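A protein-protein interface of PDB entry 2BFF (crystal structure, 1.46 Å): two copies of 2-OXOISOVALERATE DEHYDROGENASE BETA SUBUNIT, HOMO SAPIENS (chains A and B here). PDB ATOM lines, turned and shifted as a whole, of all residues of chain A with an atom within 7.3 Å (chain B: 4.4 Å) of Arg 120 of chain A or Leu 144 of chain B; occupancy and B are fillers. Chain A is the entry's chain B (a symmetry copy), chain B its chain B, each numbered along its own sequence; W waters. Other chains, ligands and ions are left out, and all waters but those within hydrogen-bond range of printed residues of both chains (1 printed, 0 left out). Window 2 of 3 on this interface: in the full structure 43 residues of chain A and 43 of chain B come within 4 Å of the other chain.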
ATOM      1  N   ILE A  84     -31.361  -3.287  -3.609  1.00  0.00           N
ATOM      2  CA  ILE A  84     -29.916  -3.529  -3.350  1.00  0.00           C
ATOM      3  C   ILE A  84     -29.386  -2.449  -2.404  1.00  0.00           C
ATOM      4  O   ILE A  84     -28.634  -2.718  -1.474  1.00  0.00           O
ATOM      5  CB  ILE A  84     -29.146  -3.493  -4.660  1.00  0.00           C
ATOM      6  CG1 ILE A  84     -29.458  -4.721  -5.502  1.00  0.00           C
ATOM      7  CG2 ILE A  84     -27.607  -3.358  -4.431  1.00  0.00           C
ATOM      8  CD1 ILE A  84     -29.017  -4.702  -7.001  1.00  0.00           C
ATOM      9  N   VAL A 111     -28.009  -9.408 -12.232  1.00  0.00           N
ATOM     10  CA  VAL A 111     -26.855 -10.211 -12.652  1.00  0.00           C
ATOM     11  C   VAL A 111     -25.573  -9.413 -12.547  1.00  0.00           C
ATOM     12  O   VAL A 111     -24.536  -9.950 -12.056  1.00  0.00           O
ATOM     13  CB  VAL A 111     -27.110 -10.741 -14.064  1.00  0.00           C
ATOM     14  CG1 VAL A 111     -25.831 -11.247 -14.737  1.00  0.00           C
ATOM     15  CG2 VAL A 111     -28.241 -11.823 -14.054  1.00  0.00           C
ATOM     16  N   ASN A 112     -25.558  -8.154 -12.994  1.00  0.00           N
ATOM     17  CA  ASN A 112     -24.298  -7.408 -12.959  1.00  0.00           C
ATOM     18  C   ASN A 112     -24.064  -6.796 -11.582  1.00  0.00           C
ATOM     19  O   ASN A 112     -22.922  -6.542 -11.239  1.00  0.00           O
ATOM     20  CB  ASN A 112     -24.288  -6.303 -14.025  1.00  0.00           C
ATOM     21  CG  ASN A 112     -23.612  -6.759 -15.324  1.00  0.00           C
ATOM     22  OD1 ASN A 112     -22.864  -7.766 -15.282  1.00  0.00           O
ATOM     23  ND2 ASN A 112     -23.805  -6.022 -16.411  1.00  0.00           N
ATOM     24  N   GLU A 113     -25.142  -6.508 -10.841  1.00  0.00           N
ATOM     25  CA  GLU A 113     -24.948  -5.830  -9.557  1.00  0.00           C
ATOM     26  C   GLU A 113     -25.147  -6.749  -8.349  1.00  0.00           C
ATOM     27  O   GLU A 113     -24.194  -7.090  -7.660  1.00  0.00           O
ATOM     28  CB  GLU A 113     -25.850  -4.565  -9.443  1.00  0.00           C
ATOM     29  CG  GLU A 113     -25.470  -3.535 -10.523  1.00  0.00           C
ATOM     30  CD  GLU A 113     -24.194  -2.794 -10.168  1.00  0.00           C
ATOM     31  OE1 GLU A 113     -24.126  -2.283  -9.058  1.00  0.00           O
ATOM     32  OE2 GLU A 113     -23.265  -2.721 -11.027  1.00  0.00           O
ATOM     33  N   ALA A 114     -26.409  -7.157  -8.098  1.00  0.00           N
ATOM     34  CA  ALA A 114     -26.649  -7.924  -6.858  1.00  0.00           C
ATOM     35  C   ALA A 114     -25.729  -9.136  -6.740  1.00  0.00           C
ATOM     36  O   ALA A 114     -25.168  -9.406  -5.664  1.00  0.00           O
ATOM     37  CB  ALA A 114     -28.132  -8.364  -6.809  1.00  0.00           C
ATOM     38  N   ALA A 115     -25.652  -9.911  -7.820  1.00  0.00           N
ATOM     39  CA  ALA A 115     -24.907 -11.169  -7.685  1.00  0.00           C
ATOM     40  C   ALA A 115     -23.424 -10.983  -7.454  1.00  0.00           C
ATOM     41  O   ALA A 115     -22.765 -11.859  -6.883  1.00  0.00           O
ATOM     42  CB  ALA A 115     -25.083 -11.957  -9.007  1.00  0.00           C
ATOM     43  N   LYS A 116     -22.906  -9.831  -7.938  1.00  0.00           N
ATOM     44  CA  LYS A 116     -21.467  -9.575  -7.927  1.00  0.00           C
ATOM     45  C   LYS A 116     -21.007  -8.622  -6.846  1.00  0.00           C
ATOM     46  O   LYS A 116     -19.792  -8.398  -6.694  1.00  0.00           O
ATOM     47  CB  LYS A 116     -21.033  -9.075  -9.285  1.00  0.00           C
ATOM     48  CG  LYS A 116     -21.163 -10.168 -10.403  1.00  0.00           C
ATOM     49  CD  LYS A 116     -21.096  -9.504 -11.822  1.00  0.00           C
ATOM     50  CE  LYS A 116     -21.082 -10.571 -12.948  1.00  0.00           C
ATOM     51  NZ  LYS A 116     -22.320 -11.482 -12.864  1.00  0.00           N
ATOM     52  N   TYR A 117     -21.967  -8.157  -6.038  1.00  0.00           N
ATOM     53  CA  TYR A 117     -21.686  -7.099  -5.088  1.00  0.00           C
ATOM     54  C   TYR A 117     -20.608  -7.466  -4.050  1.00  0.00           C
ATOM     55  O   TYR A 117     -19.708  -6.626  -3.746  1.00  0.00           O
ATOM     56  CB  TYR A 117     -23.016  -6.728  -4.343  1.00  0.00           C
ATOM     57  CG  TYR A 117     -23.244  -5.235  -4.281  1.00  0.00           C
ATOM     58  CD1 TYR A 117     -24.005  -4.619  -5.311  1.00  0.00           C
ATOM     59  CD2 TYR A 117     -22.735  -4.452  -3.228  1.00  0.00           C
ATOM     60  CE1 TYR A 117     -24.248  -3.212  -5.291  1.00  0.00           C
ATOM     61  CE2 TYR A 117     -22.947  -3.064  -3.257  1.00  0.00           C
ATOM     62  CZ  TYR A 117     -23.730  -2.460  -4.271  1.00  0.00           C
ATOM     63  OH  TYR A 117     -23.861  -1.089  -4.268  1.00  0.00           O
ATOM     64  N   ARG A 118     -20.730  -8.667  -3.477  1.00  0.00           N
ATOM     65  CA  ARG A 118     -19.812  -9.055  -2.398  1.00  0.00           C
ATOM     66  C   ARG A 118     -18.471  -9.383  -3.036  1.00  0.00           C
ATOM     67  O   ARG A 118     -17.419  -8.941  -2.555  1.00  0.00           O
ATOM     68  CB  ARG A 118     -20.430 -10.268  -1.667  1.00  0.00           C
ATOM     69  CG  ARG A 118     -19.576 -10.546  -0.399  1.00  0.00           C
ATOM     70  CD  ARG A 118     -20.029 -11.819   0.319  1.00  0.00           C
ATOM     71  NE  ARG A 118     -21.455 -11.773   0.725  1.00  0.00           N
ATOM     72  CZ  ARG A 118     -21.874 -11.283   1.922  1.00  0.00           C
ATOM     73  NH1 ARG A 118     -21.004 -10.709   2.786  1.00  0.00           N
ATOM     74  NH2 ARG A 118     -23.191 -11.316   2.223  1.00  0.00           N
ATOM     75  N   TYR A 119     -18.494 -10.138  -4.135  1.00  0.00           N
ATOM     76  CA  TYR A 119     -17.224 -10.581  -4.696  1.00  0.00           C
ATOM     77  C   TYR A 119     -16.343  -9.368  -5.126  1.00  0.00           C
ATOM     78  O   TYR A 119     -15.152  -9.264  -4.826  1.00  0.00           O
ATOM     79  CB  TYR A 119     -17.529 -11.366  -5.964  1.00  0.00           C
ATOM     80  CG  TYR A 119     -16.311 -11.980  -6.605  1.00  0.00           C
ATOM     81  CD1 TYR A 119     -15.737 -13.131  -6.061  1.00  0.00           C
ATOM     82  CD2 TYR A 119     -15.805 -11.461  -7.820  1.00  0.00           C
ATOM     83  CE1 TYR A 119     -14.639 -13.794  -6.703  1.00  0.00           C
ATOM     84  CE2 TYR A 119     -14.710 -12.093  -8.434  1.00  0.00           C
ATOM     85  CZ  TYR A 119     -14.180 -13.271  -7.864  1.00  0.00           C
ATOM     86  OH  TYR A 119     -13.100 -13.905  -8.496  1.00  0.00           O
ATOM     87  N   ARG A 120     -16.981  -8.438  -5.845  1.00  0.00           N
ATOM     88  CA  ARG A 120     -16.224  -7.419  -6.500  1.00  0.00           C
ATOM     89  C   ARG A 120     -15.698  -6.380  -5.514  1.00  0.00           C
ATOM     90  O   ARG A 120     -14.786  -5.568  -5.845  1.00  0.00           O
ATOM     91  CB  ARG A 120     -17.069  -6.742  -7.574  1.00  0.00           C
ATOM     92  CG  ARG A 120     -18.046  -5.723  -7.005  1.00  0.00           C
ATOM     93  CD  ARG A 120     -19.086  -5.324  -8.020  1.00  0.00           C
ATOM     94  NE  ARG A 120     -19.999  -4.337  -7.441  1.00  0.00           N
ATOM     95  CZ  ARG A 120     -21.061  -3.847  -8.102  1.00  0.00           C
ATOM     96  NH1 ARG A 120     -21.393  -4.360  -9.348  1.00  0.00           N
ATOM     97  NH2 ARG A 120     -21.810  -2.886  -7.521  1.00  0.00           N
ATOM     98  N   SER A 121     -16.275  -6.346  -4.315  1.00  0.00           N
ATOM     99  CA  SER A 121     -15.793  -5.439  -3.308  1.00  0.00           C
ATOM    100  C   SER A 121     -14.827  -6.080  -2.321  1.00  0.00           C
ATOM    101  O   SER A 121     -14.435  -5.416  -1.346  1.00  0.00           O
ATOM    102  CB  SER A 121     -16.982  -4.839  -2.538  1.00  0.00           C
ATOM    103  OG  SER A 121     -17.603  -5.835  -1.713  1.00  0.00           O
ATOM    104  N   GLY A 122     -14.468  -7.344  -2.540  1.00  0.00           N
ATOM    105  CA  GLY A 122     -13.679  -8.070  -1.521  1.00  0.00           C
ATOM    106  C   GLY A 122     -14.378  -8.209  -0.157  1.00  0.00           C
ATOM    107  O   GLY A 122     -13.745  -8.316   0.903  1.00  0.00           O
ATOM    108  N   ASP A 123     -15.724  -8.237  -0.229  1.00  0.00           N
ATOM    109  CA  ASP A 123     -16.551  -8.315   0.986  1.00  0.00           C
ATOM    110  C   ASP A 123     -16.506  -7.012   1.801  1.00  0.00           C
ATOM    111  O   ASP A 123     -16.881  -7.017   2.990  1.00  0.00           O
ATOM    112  CB  ASP A 123     -16.187  -9.542   1.879  1.00  0.00           C
ATOM    113  CG  ASP A 123     -17.299  -9.834   2.882  1.00  0.00           C
ATOM    114  OD1 ASP A 123     -18.485  -9.633   2.557  1.00  0.00           O
ATOM    115  OD2 ASP A 123     -17.026 -10.168   4.089  1.00  0.00           O
ATOM    116  N   LEU A 124     -16.144  -5.878   1.169  1.00  0.00           N
ATOM    117  CA  LEU A 124     -16.304  -4.588   1.867  1.00  0.00           C
ATOM    118  C   LEU A 124     -17.778  -4.177   1.869  1.00  0.00           C
ATOM    119  O   LEU A 124     -18.179  -3.477   2.790  1.00  0.00           O
ATOM    120  CB  LEU A 124     -15.446  -3.475   1.224  1.00  0.00           C
ATOM    121  CG  LEU A 124     -13.923  -3.575   1.460  1.00  0.00           C
ATOM    122  CD1 LEU A 124     -13.340  -2.314   0.832  1.00  0.00           C
ATOM    123  CD2 LEU A 124     -13.575  -3.690   2.902  1.00  0.00           C
ATOM    124  N   PHE A 125     -18.526  -4.584   0.829  1.00  0.00           N
ATOM    125  CA  PHE A 125     -19.981  -4.258   0.786  1.00  0.00           C
ATOM    126  C   PHE A 125     -20.715  -5.508   0.333  1.00  0.00           C
ATOM    127  O   PHE A 125     -20.119  -6.373  -0.342  1.00  0.00           O
ATOM    128  CB  PHE A 125     -20.249  -3.107  -0.218  1.00  0.00           C
ATOM    129  CG  PHE A 125     -19.573  -1.833   0.204  1.00  0.00           C
ATOM    130  CD1 PHE A 125     -20.202  -0.974   1.083  1.00  0.00           C
ATOM    131  CD2 PHE A 125     -18.297  -1.526  -0.263  1.00  0.00           C
ATOM    132  CE1 PHE A 125     -19.582   0.207   1.500  1.00  0.00           C
ATOM    133  CE2 PHE A 125     -17.666  -0.364   0.195  1.00  0.00           C
ATOM    134  CZ  PHE A 125     -18.296   0.477   1.049  1.00  0.00           C
ATOM    135  N   ASP B 101     -20.980  -7.321 -21.871  1.00  0.00           N
ATOM    136  CA  ASP B 101     -21.239  -7.218 -20.433  1.00  0.00           C
ATOM    137  C   ASP B 101     -22.363  -6.237 -20.192  1.00  0.00           C
ATOM    138  O   ASP B 101     -22.977  -6.271 -19.119  1.00  0.00           O
ATOM    139  CB  ASP B 101     -19.955  -6.695 -19.782  1.00  0.00           C
ATOM    140  CG  ASP B 101     -18.749  -7.515 -20.167  1.00  0.00           C
ATOM    141  OD1 ASP B 101     -18.315  -7.396 -21.346  1.00  0.00           O
ATOM    142  OD2 ASP B 101     -18.213  -8.246 -19.318  1.00  0.00           O
ATOM    143  N   GLY B 142      -9.815  -7.723 -18.619  1.00  0.00           N
ATOM    144  CA  GLY B 142     -11.125  -7.044 -18.655  1.00  0.00           C
ATOM    145  C   GLY B 142     -11.929  -7.156 -17.334  1.00  0.00           C
ATOM    146  O   GLY B 142     -12.896  -6.403 -17.151  1.00  0.00           O
ATOM    147  N   ALA B 143     -11.552  -8.072 -16.475  1.00  0.00           N
ATOM    148  CA  ALA B 143     -12.238  -8.250 -15.181  1.00  0.00           C
ATOM    149  C   ALA B 143     -13.750  -8.491 -15.394  1.00  0.00           C
ATOM    150  O   ALA B 143     -14.168  -9.148 -16.363  1.00  0.00           O
ATOM    151  CB  ALA B 143     -11.906  -7.076 -14.234  1.00  0.00           C
ATOM    152  N   LEU B 144     -14.556  -7.949 -14.481  1.00  0.00           N
ATOM    153  CA  LEU B 144     -15.914  -8.479 -14.375  1.00  0.00           C
ATOM    154  C   LEU B 144     -16.791  -8.032 -15.523  1.00  0.00           C
ATOM    155  O   LEU B 144     -17.759  -8.723 -15.872  1.00  0.00           O
ATOM    156  CB  LEU B 144     -16.590  -8.012 -13.067  1.00  0.00           C
ATOM    157  CG  LEU B 144     -16.294  -8.867 -11.831  1.00  0.00           C
ATOM    158  CD1 LEU B 144     -14.848  -8.666 -11.281  1.00  0.00           C
ATOM    159  CD2 LEU B 144     -17.289  -8.558 -10.768  1.00  0.00           C
ATOM    160  N   TYR B 145     -16.492  -6.849 -16.065  1.00  0.00           N
ATOM    161  CA  TYR B 145     -17.432  -6.168 -16.954  1.00  0.00           C
ATOM    162  C   TYR B 145     -16.864  -5.859 -18.331  1.00  0.00           C
ATOM    163  O   TYR B 145     -17.546  -5.148 -19.131  1.00  0.00           O
ATOM    164  CB  TYR B 145     -18.070  -4.908 -16.316  1.00  0.00           C
ATOM    165  CG  TYR B 145     -18.660  -5.196 -14.952  1.00  0.00           C
ATOM    166  CD1 TYR B 145     -19.859  -5.919 -14.875  1.00  0.00           C
ATOM    167  CD2 TYR B 145     -18.030  -4.803 -13.771  1.00  0.00           C
ATOM    168  CE1 TYR B 145     -20.420  -6.247 -13.653  1.00  0.00           C
ATOM    169  CE2 TYR B 145     -18.589  -5.108 -12.533  1.00  0.00           C
ATOM    170  CZ  TYR B 145     -19.798  -5.824 -12.509  1.00  0.00           C
ATOM    171  OH  TYR B 145     -20.318  -6.132 -11.260  1.00  0.00           O
ATOM    172  N   HIS B 146     -15.674  -6.393 -18.634  1.00  0.00           N
ATOM    173  CA  HIS B 146     -15.133  -6.265 -19.998  1.00  0.00           C
ATOM    174  C   HIS B 146     -14.812  -7.627 -20.608  1.00  0.00           C
ATOM    175  O   HIS B 146     -14.206  -7.706 -21.660  1.00  0.00           O
ATOM    176  CB  HIS B 146     -13.864  -5.424 -19.991  1.00  0.00           C
ATOM    177  CG  HIS B 146     -14.116  -3.954 -20.157  1.00  0.00           C
ATOM    178  ND1 HIS B 146     -13.076  -3.081 -20.412  1.00  0.00           N
ATOM    179  CD2 HIS B 146     -15.244  -3.198 -20.142  1.00  0.00           C
ATOM    180  CE1 HIS B 146     -13.558  -1.845 -20.498  1.00  0.00           C
ATOM    181  NE2 HIS B 146     -14.877  -1.894 -20.351  1.00  0.00           N
ATOM    182  N   GLN B 148     -17.201 -10.668 -20.229  1.00  0.00           N
ATOM    183  CA  GLN B 148     -18.235 -11.723 -20.160  1.00  0.00           C
ATOM    184  C   GLN B 148     -18.556 -12.393 -21.472  1.00  0.00           C
ATOM    185  O   GLN B 148     -18.378 -11.820 -22.578  1.00  0.00           O
ATOM    186  CB  GLN B 148     -19.532 -11.160 -19.535  1.00  0.00           C
ATOM    187  CG  GLN B 148     -19.348 -10.837 -18.049  1.00  0.00           C
ATOM    188  CD  GLN B 148     -20.653 -10.352 -17.417  1.00  0.00           C
ATOM    189  OE1 GLN B 148     -21.679 -11.066 -17.534  1.00  0.00           O
ATOM    190  NE2 GLN B 148     -20.610  -9.193 -16.734  1.00  0.00           N
ATOM    191  N   PRO B 316     -17.707 -14.610 -10.741  1.00  0.00           N
ATOM    192  CA  PRO B 316     -17.573 -13.475 -11.687  1.00  0.00           C
ATOM    193  C   PRO B 316     -16.154 -13.529 -12.314  1.00  0.00           C
ATOM    194  O   PRO B 316     -15.258 -14.251 -11.828  1.00  0.00           O
ATOM    195  CB  PRO B 316     -17.790 -12.242 -10.774  1.00  0.00           C
ATOM    196  CG  PRO B 316     -18.533 -12.819  -9.566  1.00  0.00           C
ATOM    197  CD  PRO B 316     -17.874 -14.202  -9.348  1.00  0.00           C
ATOM    198  N   PHE B 317     -15.968 -12.773 -13.382  1.00  0.00           N
ATOM    199  CA  PHE B 317     -14.715 -12.894 -14.126  1.00  0.00           C
ATOM    200  C   PHE B 317     -13.645 -11.988 -13.518  1.00  0.00           C
ATOM    201  O   PHE B 317     -13.812 -10.777 -13.534  1.00  0.00           O
ATOM    202  CB  PHE B 317     -14.969 -12.545 -15.606  1.00  0.00           C
ATOM    203  CG  PHE B 317     -13.854 -13.035 -16.503  1.00  0.00           C
ATOM    204  CD1 PHE B 317     -12.597 -12.493 -16.429  1.00  0.00           C
ATOM    205  CD2 PHE B 317     -14.101 -14.104 -17.332  1.00  0.00           C
ATOM    206  CE1 PHE B 317     -11.530 -13.020 -17.183  1.00  0.00           C
ATOM    207  CE2 PHE B 317     -13.090 -14.602 -18.127  1.00  0.00           C
ATOM    208  CZ  PHE B 317     -11.812 -14.056 -18.078  1.00  0.00           C
HETATM  209  O   HOH W   1     -22.477 -12.637 -15.362  1.00  0.00           O
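Of the printed residues of chain B, Lys 116 of chain A touches Tyr 145 (3.5 Å) and Pro 316 (3.8 Å).
Of chain B, only Leu 144 and Tyr 145 come within 4 Å of Arg 120 of chain A.
Printed residues of chain A within 4 Å of Leu 144 of chain B: Arg 120.
Of the printed residues of chain A, Tyr 145 of chain B touches Asn 112 (2.6 Å), Lys 116 (3.5 Å) and Arg 120 (2.8 Å).
The nearest printed residue of chain B that does not touch Arg 120 of chain A is Pro 316 of chain B (6.0 Å).
The nearest residue of chain A that does not touch Leu 144 of chain B is Lys 116 of chain A (4.1 Å).
The side-chain carboxylate (OD2) of Asp 101 of chain B lies within hydrogen-bond range of the backbone NH (N) of His 146 of chain B, 3.2 Å away.
O of Asn 112 of chain A sits at hydrogen-bond distance from NH1 of Arg 120 of chain A, 3.3 Å away.
The guanidinium group of Arg 120 of chain A lies within salt-bridge range of the side-chain carboxylate of Glu 113 of chain A (2.8 Å).
The backbone carbonyl oxygen of Val 111 of chain A sits at hydrogen-bond distance from the side-chain amino group of Lys 116 of chain A, at 2.8 Å.
O of Leu 144 of chain B is in hydrogen-bond range of NE2 of Gln 148 of chain B, 3.0 Å away.
The backbone NH (N) of Leu 144 of chain B sits at hydrogen-bond distance from the backbone carbonyl oxygen (O) of Phe 317 of chain B (3.1 Å).
Water W1 bridges NZ of Lys 116 of chain A (2.8 Å) and OE1 of Gln 148 of chain B (2.8 Å).
No position is printed for both chains.
Among the printed residues, merely in contact across the chains: Lys 116 of chain A with Tyr 145 of chain B, Tyr 119 of chain A with Pro 316 of chain B, Arg 120 of chain A with Leu 144 of chain B and Lys 116 of chain A with Pro 316 of chain B.
Of the 9 printed residues of chain B, 5 touch a printed residue of chain A.
Printed residues of chain B that touch a printed residue of chain A: Asp 101, Leu 144, Tyr 145, Gln 148 and Pro 316.
The backbone carbonyl oxygen of Asn 112 of chain A sits at hydrogen-bond distance from the side-chain hydroxyl of Tyr 145 of chain B (2.6 Å).
The side-chain amide nitrogen (ND2) of Asn 112 of chain A sits at hydrogen-bond distance from the backbone carbonyl oxygen (O) of Asp 101 of chain B (2.8 Å).
OH of Tyr 145 of chain B is in hydrogen-bond range of NH1 of Arg 120 of chain A (2.8 Å).
The side-chain amide nitrogen (NE2) of Gln 148 of chain B lies within hydrogen-bond range of the side-chain amide oxygen (OD1) of Asn 112 of chain A, 3.0 Å away.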
